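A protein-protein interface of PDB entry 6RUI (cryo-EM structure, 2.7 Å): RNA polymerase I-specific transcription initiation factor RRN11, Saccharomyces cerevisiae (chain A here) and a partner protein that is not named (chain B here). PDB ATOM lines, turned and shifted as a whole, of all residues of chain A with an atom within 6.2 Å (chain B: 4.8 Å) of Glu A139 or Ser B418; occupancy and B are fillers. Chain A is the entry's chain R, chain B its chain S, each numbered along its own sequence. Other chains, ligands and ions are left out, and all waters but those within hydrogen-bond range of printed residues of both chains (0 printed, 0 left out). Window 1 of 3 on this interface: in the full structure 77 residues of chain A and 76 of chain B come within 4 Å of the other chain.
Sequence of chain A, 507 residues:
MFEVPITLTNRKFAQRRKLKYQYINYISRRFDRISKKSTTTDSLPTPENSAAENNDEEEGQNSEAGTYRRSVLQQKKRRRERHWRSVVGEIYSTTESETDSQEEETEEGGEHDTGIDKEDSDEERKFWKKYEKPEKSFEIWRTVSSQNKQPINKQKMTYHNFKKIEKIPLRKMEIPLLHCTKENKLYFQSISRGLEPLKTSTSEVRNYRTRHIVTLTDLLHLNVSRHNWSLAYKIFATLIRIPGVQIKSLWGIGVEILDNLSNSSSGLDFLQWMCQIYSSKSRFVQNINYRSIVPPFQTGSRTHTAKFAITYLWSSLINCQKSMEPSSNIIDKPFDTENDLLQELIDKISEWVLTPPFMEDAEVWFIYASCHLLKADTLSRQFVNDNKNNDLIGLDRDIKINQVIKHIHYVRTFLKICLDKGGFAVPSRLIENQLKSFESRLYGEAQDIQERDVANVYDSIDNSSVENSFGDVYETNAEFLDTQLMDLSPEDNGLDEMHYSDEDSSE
The side-chain carboxylate of Glu A139 sits at hydrogen-bond distance from the side-chain hydroxyl of Ser B418, 2.6 Å away. OG of Ser B400 lies within hydrogen-bond range of OE2 of Glu A139, at 2.8 Å. The backbone carbonyl oxygen (O) of Gln B395 is in hydrogen-bond range of the backbone NH (N) of Ile A140 (3.1 Å).
The side-chain hydroxyl (OG) of Ser B418 is in hydrogen-bond range of the side-chain hydroxyl (OG) of Ser B400 (3.5 Å). The backbone NH (N) of Glu A139 sits close to the side-chain hydroxyl (OG) of Ser A137 (3.5 Å). The backbone carbonyl oxygen of Ala B396 lies close to the side-chain amide oxygen of Asn B401. The backbone carbonyl oxygen (O) of Glu B420 is in hydrogen-bond range of the backbone NH (N) of Leu B442 (3.5 Å). The side-chain hydroxyl (OG) of Ser B418 is in hydrogen-bond range of the backbone carbonyl oxygen (O) of Asn B401. N of Leu B416 is in hydrogen-bond range of O of Ile B423, at 2.5 Å.
OE1 of Glu B420 touches CD1 of Phe A138 (3.6 Å). Ile B421 touches Phe A138 (CD1 to CE2, 3.4 Å). Glu A139 touches Val B394 (OE1 to CG1, 3.4 Å). Glu A139 touches Gln B395 (CA to O, 3.5 Å). Ala B396 touches Glu A139 (CB to CG, 3.7 Å). Trp A141 touches Val B394 (CZ3 to CG2, 3.5 Å). Ile B423 touches Trp A141.
Of chain B, only Val B394, Gln B395, Ala B396, Ser B400 and Ser B418 come within 4 Å of Glu A139. Of the printed residues of chain B, Trp A141 touches Val B394 (3.5 Å) and Ile B423 (3.5 Å). Of the printed residues of chain A, Val B394 touches Glu A139 and Trp A141. Ser B418 touches just one residue of chain A: Glu A139 (2.6 Å). The nearest residue of chain B that does not touch Glu A139 is Ile B423 (4.1 Å). The nearest residue of chain A that does not touch Ser B418 is Phe A138 (5.9 Å).
Of the 15 printed residues of chain B, 8 touch a printed residue of chain A. Hydrophobic or aromatic side chains of chain B that line the printed part of chain A: Val B394, Ala B396, Ile B421 and Ile B423. Of the 7 printed residues of chain A, 4 touch a printed residue of chain B. Hydrophobic or aromatic side chains of chain A within 4 Å of the printed part of chain B: Phe A138, Ile A140 and Trp A141. Among the printed residues, 10 pairs touch across the chains. Among the printed residues, no Asp or Glu carboxylate lies within 4 Å of a Lys or Arg side-chain nitrogen of the other chain.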
ATOM      1  N   PRO A 134      34.866 -22.916 -30.691  1.00  0.00           N
ATOM      2  CA  PRO A 134      35.796 -23.660 -29.823  1.00  0.00           C
ATOM      3  C   PRO A 134      36.919 -24.422 -30.503  1.00  0.00           C
ATOM      4  O   PRO A 134      38.071 -24.330 -30.062  1.00  0.00           O
ATOM      5  CB  PRO A 134      34.866 -24.638 -29.101  1.00  0.00           C
ATOM      6  CG  PRO A 134      33.579 -23.954 -29.073  1.00  0.00           C
ATOM      7  CD  PRO A 134      33.467 -23.183 -30.332  1.00  0.00           C
ATOM      8  N   SER A 137      36.866 -28.552 -28.476  1.00  0.00           N
ATOM      9  CA  SER A 137      35.673 -29.228 -28.006  1.00  0.00           C
ATOM     10  C   SER A 137      34.468 -28.776 -28.812  1.00  0.00           C
ATOM     11  O   SER A 137      34.559 -27.898 -29.671  1.00  0.00           O
ATOM     12  CB  SER A 137      35.451 -28.964 -26.517  1.00  0.00           C
ATOM     13  OG  SER A 137      35.190 -27.597 -26.276  1.00  0.00           O
ATOM     14  N   PHE A 138      33.330 -29.416 -28.543  1.00  0.00           N
ATOM     15  CA  PHE A 138      32.078 -28.949 -29.120  1.00  0.00           C
ATOM     16  C   PHE A 138      31.713 -27.586 -28.573  1.00  0.00           C
ATOM     17  O   PHE A 138      31.298 -26.691 -29.315  1.00  0.00           O
ATOM     18  CB  PHE A 138      30.953 -29.948 -28.845  1.00  0.00           C
ATOM     19  CG  PHE A 138      31.159 -31.286 -29.497  1.00  0.00           C
ATOM     20  CD1 PHE A 138      30.807 -31.489 -30.821  1.00  0.00           C
ATOM     21  CD2 PHE A 138      31.704 -32.342 -28.785  1.00  0.00           C
ATOM     22  CE1 PHE A 138      30.996 -32.719 -31.423  1.00  0.00           C
ATOM     23  CE2 PHE A 138      31.895 -33.573 -29.381  1.00  0.00           C
ATOM     24  CZ  PHE A 138      31.541 -33.763 -30.703  1.00  0.00           C
ATOM     25  N   GLU A 139      31.853 -27.434 -27.270  1.00  0.00           N
ATOM     26  CA  GLU A 139      31.339 -26.322 -26.501  1.00  0.00           C
ATOM     27  C   GLU A 139      32.521 -25.683 -25.813  1.00  0.00           C
ATOM     28  O   GLU A 139      33.433 -26.381 -25.372  1.00  0.00           O
ATOM     29  CB  GLU A 139      30.352 -26.837 -25.482  1.00  0.00           C
ATOM     30  CG  GLU A 139      29.233 -27.563 -26.150  1.00  0.00           C
ATOM     31  CD  GLU A 139      28.500 -28.487 -25.233  1.00  0.00           C
ATOM     32  OE1 GLU A 139      28.942 -28.639 -24.078  1.00  0.00           O
ATOM     33  OE2 GLU A 139      27.507 -29.097 -25.679  1.00  0.00           O
ATOM     34  N   ILE A 140      32.530 -24.365 -25.722  1.00  0.00           N
ATOM     35  CA  ILE A 140      33.723 -23.775 -25.147  1.00  0.00           C
ATOM     36  C   ILE A 140      33.593 -23.829 -23.628  1.00  0.00           C
ATOM     37  O   ILE A 140      33.098 -22.906 -22.976  1.00  0.00           O
ATOM     38  CB  ILE A 140      34.007 -22.376 -25.744  1.00  0.00           C
ATOM     39  CG1 ILE A 140      35.256 -21.753 -25.125  1.00  0.00           C
ATOM     40  CG2 ILE A 140      32.776 -21.485 -25.829  1.00  0.00           C
ATOM     41  CD1 ILE A 140      35.817 -20.629 -25.933  1.00  0.00           C
ATOM     42  N   TRP A 141      34.000 -24.968 -23.074  1.00  0.00           N
ATOM     43  CA  TRP A 141      34.087 -25.194 -21.643  1.00  0.00           C
ATOM     44  C   TRP A 141      35.138 -24.287 -21.031  1.00  0.00           C
ATOM     45  O   TRP A 141      36.065 -23.826 -21.699  1.00  0.00           O
ATOM     46  CB  TRP A 141      34.469 -26.638 -21.351  1.00  0.00           C
ATOM     47  CG  TRP A 141      33.436 -27.625 -21.669  1.00  0.00           C
ATOM     48  CD1 TRP A 141      33.229 -28.228 -22.864  1.00  0.00           C
ATOM     49  CD2 TRP A 141      32.519 -28.209 -20.761  1.00  0.00           C
ATOM     50  NE1 TRP A 141      32.196 -29.118 -22.773  1.00  0.00           N
ATOM     51  CE2 TRP A 141      31.744 -29.127 -21.484  1.00  0.00           C
ATOM     52  CE3 TRP A 141      32.256 -28.029 -19.408  1.00  0.00           C
ATOM     53  CZ2 TRP A 141      30.728 -29.859 -20.900  1.00  0.00           C
ATOM     54  CZ3 TRP A 141      31.239 -28.757 -18.832  1.00  0.00           C
ATOM     55  CH2 TRP A 141      30.495 -29.666 -19.571  1.00  0.00           C
ATOM     56  N   PRO A 296      35.651 -30.809 -33.880  1.00  0.00           N
ATOM     57  CA  PRO A 296      36.226 -31.629 -32.797  1.00  0.00           C
ATOM     58  C   PRO A 296      36.389 -33.113 -33.092  1.00  0.00           C
ATOM     59  O   PRO A 296      36.969 -33.802 -32.259  1.00  0.00           O
ATOM     60  CB  PRO A 296      35.233 -31.436 -31.646  1.00  0.00           C
ATOM     61  CG  PRO A 296      34.463 -30.273 -31.993  1.00  0.00           C
ATOM     62  CD  PRO A 296      34.312 -30.370 -33.446  1.00  0.00           C
ATOM     63  N   VAL B 394      29.579 -23.933 -19.283  1.00  0.00           N
ATOM     64  CA  VAL B 394      29.313 -24.404 -20.635  1.00  0.00           C
ATOM     65  C   VAL B 394      28.867 -23.203 -21.442  1.00  0.00           C
ATOM     66  O   VAL B 394      28.170 -22.325 -20.928  1.00  0.00           O
ATOM     67  CB  VAL B 394      28.241 -25.511 -20.653  1.00  0.00           C
ATOM     68  CG1 VAL B 394      28.058 -26.106 -22.043  1.00  0.00           C
ATOM     69  CG2 VAL B 394      28.577 -26.588 -19.669  1.00  0.00           C
ATOM     70  N   GLN B 395      29.312 -23.149 -22.701  1.00  0.00           N
ATOM     71  CA  GLN B 395      28.926 -22.143 -23.733  1.00  0.00           C
ATOM     72  C   GLN B 395      28.635 -23.007 -24.957  1.00  0.00           C
ATOM     73  O   GLN B 395      29.597 -23.398 -25.629  1.00  0.00           O
ATOM     74  CB  GLN B 395      30.060 -21.160 -24.018  1.00  0.00           C
ATOM     75  CG  GLN B 395      29.606 -19.710 -24.085  1.00  0.00           C
ATOM     76  CD  GLN B 395      29.737 -19.118 -25.466  1.00  0.00           C
ATOM     77  OE1 GLN B 395      30.725 -18.469 -25.796  1.00  0.00           O
ATOM     78  NE2 GLN B 395      28.725 -19.334 -26.289  1.00  0.00           N
ATOM     79  N   ALA B 396      27.363 -23.252 -25.261  1.00  0.00           N
ATOM     80  CA  ALA B 396      27.086 -24.307 -26.226  1.00  0.00           C
ATOM     81  C   ALA B 396      26.362 -23.750 -27.435  1.00  0.00           C
ATOM     82  O   ALA B 396      25.316 -24.265 -27.831  1.00  0.00           O
ATOM     83  CB  ALA B 396      26.262 -25.416 -25.572  1.00  0.00           C
ATOM     84  N   SER B 400      26.600 -27.328 -30.995  1.00  0.00           N
ATOM     85  CA  SER B 400      25.680 -28.221 -30.315  1.00  0.00           C
ATOM     86  C   SER B 400      24.660 -27.381 -29.561  1.00  0.00           C
ATOM     87  O   SER B 400      24.559 -26.173 -29.768  1.00  0.00           O
ATOM     88  CB  SER B 400      26.451 -29.184 -29.412  1.00  0.00           C
ATOM     89  OG  SER B 400      27.114 -28.469 -28.402  1.00  0.00           O
ATOM     90  N   ASN B 401      23.880 -28.041 -28.706  1.00  0.00           N
ATOM     91  CA  ASN B 401      22.909 -27.400 -27.830  1.00  0.00           C
ATOM     92  C   ASN B 401      22.690 -28.280 -26.613  1.00  0.00           C
ATOM     93  O   ASN B 401      22.806 -29.505 -26.690  1.00  0.00           O
ATOM     94  CB  ASN B 401      21.556 -27.160 -28.510  1.00  0.00           C
ATOM     95  CG  ASN B 401      21.536 -25.917 -29.372  1.00  0.00           C
ATOM     96  OD1 ASN B 401      22.074 -24.878 -28.997  1.00  0.00           O
ATOM     97  ND2 ASN B 401      20.893 -26.011 -30.525  1.00  0.00           N
ATOM     98  N   ILE B 402      22.351 -27.651 -25.494  1.00  0.00           N
ATOM     99  CA  ILE B 402      21.972 -28.392 -24.300  1.00  0.00           C
ATOM    100  C   ILE B 402      20.564 -28.932 -24.499  1.00  0.00           C
ATOM    101  O   ILE B 402      19.651 -28.189 -24.876  1.00  0.00           O
ATOM    102  CB  ILE B 402      22.053 -27.503 -23.050  1.00  0.00           C
ATOM    103  CG1 ILE B 402      23.470 -26.983 -22.838  1.00  0.00           C
ATOM    104  CG2 ILE B 402      21.641 -28.277 -21.819  1.00  0.00           C
ATOM    105  CD1 ILE B 402      23.554 -25.935 -21.755  1.00  0.00           C
ATOM    106  N   ARG B 403      20.382 -30.228 -24.251  1.00  0.00           N
ATOM    107  CA  ARG B 403      19.112 -30.896 -24.490  1.00  0.00           C
ATOM    108  C   ARG B 403      18.403 -31.319 -23.212  1.00  0.00           C
ATOM    109  O   ARG B 403      17.209 -31.057 -23.058  1.00  0.00           O
ATOM    110  CB  ARG B 403      19.332 -32.114 -25.393  1.00  0.00           C
ATOM    111  CG  ARG B 403      19.905 -31.762 -26.754  1.00  0.00           C
ATOM    112  CD  ARG B 403      18.904 -30.998 -27.578  1.00  0.00           C
ATOM    113  NE  ARG B 403      19.446 -30.572 -28.859  1.00  0.00           N
ATOM    114  CZ  ARG B 403      18.800 -29.788 -29.707  1.00  0.00           C
ATOM    115  NH1 ARG B 403      17.591 -29.349 -29.412  1.00  0.00           N
ATOM    116  NH2 ARG B 403      19.363 -29.436 -30.849  1.00  0.00           N
ATOM    117  N   LEU B 416      24.822 -34.923 -18.098  1.00  0.00           N
ATOM    118  CA  LEU B 416      24.289 -33.925 -19.017  1.00  0.00           C
ATOM    119  C   LEU B 416      24.170 -34.504 -20.420  1.00  0.00           C
ATOM    120  O   LEU B 416      25.083 -35.178 -20.900  1.00  0.00           O
ATOM    121  CB  LEU B 416      25.198 -32.696 -19.060  1.00  0.00           C
ATOM    122  CG  LEU B 416      24.904 -31.626 -20.111  1.00  0.00           C
ATOM    123  CD1 LEU B 416      23.584 -30.964 -19.854  1.00  0.00           C
ATOM    124  CD2 LEU B 416      26.018 -30.603 -20.199  1.00  0.00           C
ATOM    125  N   THR B 417      23.052 -34.232 -21.082  1.00  0.00           N
ATOM    126  CA  THR B 417      22.874 -34.584 -22.487  1.00  0.00           C
ATOM    127  C   THR B 417      22.940 -33.308 -23.305  1.00  0.00           C
ATOM    128  O   THR B 417      22.019 -32.487 -23.290  1.00  0.00           O
ATOM    129  CB  THR B 417      21.571 -35.327 -22.727  1.00  0.00           C
ATOM    130  OG1 THR B 417      21.644 -36.591 -22.076  1.00  0.00           O
ATOM    131  CG2 THR B 417      21.347 -35.568 -24.205  1.00  0.00           C
ATOM    132  N   SER B 418      24.051 -33.140 -23.997  1.00  0.00           N
ATOM    133  CA  SER B 418      24.145 -32.157 -25.049  1.00  0.00           C
ATOM    134  C   SER B 418      23.582 -32.752 -26.330  1.00  0.00           C
ATOM    135  O   SER B 418      23.249 -33.936 -26.404  1.00  0.00           O
ATOM    136  CB  SER B 418      25.596 -31.733 -25.236  1.00  0.00           C
ATOM    137  OG  SER B 418      25.735 -30.891 -26.360  1.00  0.00           O
ATOM    138  N   ARG B 419      23.471 -31.932 -27.357  1.00  0.00           N
ATOM    139  CA  ARG B 419      23.436 -32.460 -28.703  1.00  0.00           C
ATOM    140  C   ARG B 419      24.857 -32.893 -29.008  1.00  0.00           C
ATOM    141  O   ARG B 419      25.806 -32.276 -28.514  1.00  0.00           O
ATOM    142  CB  ARG B 419      22.953 -31.419 -29.708  1.00  0.00           C
ATOM    143  CG  ARG B 419      22.741 -31.965 -31.105  1.00  0.00           C
ATOM    144  CD  ARG B 419      22.239 -30.896 -32.051  1.00  0.00           C
ATOM    145  NE  ARG B 419      23.242 -29.866 -32.309  1.00  0.00           N
ATOM    146  CZ  ARG B 419      22.999 -28.750 -32.989  1.00  0.00           C
ATOM    147  NH1 ARG B 419      23.959 -27.864 -33.188  1.00  0.00           N
ATOM    148  NH2 ARG B 419      21.789 -28.520 -33.474  1.00  0.00           N
ATOM    149  N   GLU B 420      24.998 -34.001 -29.723  1.00  0.00           N
ATOM    150  CA  GLU B 420      26.220 -34.544 -30.301  1.00  0.00           C
ATOM    151  C   GLU B 420      27.172 -35.164 -29.273  1.00  0.00           C
ATOM    152  O   GLU B 420      28.103 -35.850 -29.685  1.00  0.00           O
ATOM    153  CB  GLU B 420      26.992 -33.508 -31.148  1.00  0.00           C
ATOM    154  CG  GLU B 420      26.276 -33.159 -32.450  1.00  0.00           C
ATOM    155  CD  GLU B 420      26.896 -31.991 -33.158  1.00  0.00           C
ATOM    156  OE1 GLU B 420      27.670 -31.284 -32.504  1.00  0.00           O
ATOM    157  OE2 GLU B 420      26.656 -31.797 -34.364  1.00  0.00           O
ATOM    158  N   ILE B 421      26.942 -35.023 -27.965  1.00  0.00           N
ATOM    159  CA  ILE B 421      27.795 -35.683 -26.976  1.00  0.00           C
ATOM    160  C   ILE B 421      27.003 -35.887 -25.683  1.00  0.00           C
ATOM    161  O   ILE B 421      26.081 -35.128 -25.372  1.00  0.00           O
ATOM    162  CB  ILE B 421      29.106 -34.881 -26.774  1.00  0.00           C
ATOM    163  CG1 ILE B 421      30.196 -35.752 -26.159  1.00  0.00           C
ATOM    164  CG2 ILE B 421      28.867 -33.615 -25.981  1.00  0.00           C
ATOM    165  CD1 ILE B 421      31.572 -35.271 -26.466  1.00  0.00           C
ATOM    166  N   ILE B 423      27.495 -36.242 -21.604  1.00  0.00           N
ATOM    167  CA  ILE B 423      28.492 -35.755 -20.655  1.00  0.00           C
ATOM    168  C   ILE B 423      28.084 -36.153 -19.245  1.00  0.00           C
ATOM    169  O   ILE B 423      26.946 -35.912 -18.834  1.00  0.00           O
ATOM    170  CB  ILE B 423      28.655 -34.233 -20.767  1.00  0.00           C
ATOM    171  CG1 ILE B 423      29.081 -33.870 -22.178  1.00  0.00           C
ATOM    172  CG2 ILE B 423      29.692 -33.732 -19.800  1.00  0.00           C
ATOM    173  CD1 ILE B 423      28.912 -32.441 -22.498  1.00  0.00           C
ATOM    174  N   LEU B 442      27.710 -39.153 -28.605  1.00  0.00           N
ATOM    175  CA  LEU B 442      26.583 -39.891 -29.146  1.00  0.00           C
ATOM    176  C   LEU B 442      26.352 -39.482 -30.592  1.00  0.00           C
ATOM    177  O   LEU B 442      26.606 -38.345 -30.999  1.00  0.00           O
ATOM    178  CB  LEU B 442      25.303 -39.686 -28.338  1.00  0.00           C
ATOM    179  CG  LEU B 442      24.293 -38.583 -28.639  1.00  0.00           C
ATOM    180  CD1 LEU B 442      22.968 -39.017 -28.093  1.00  0.00           C
ATOM    181  CD2 LEU B 442      24.633 -37.315 -28.005  1.00  0.00           C
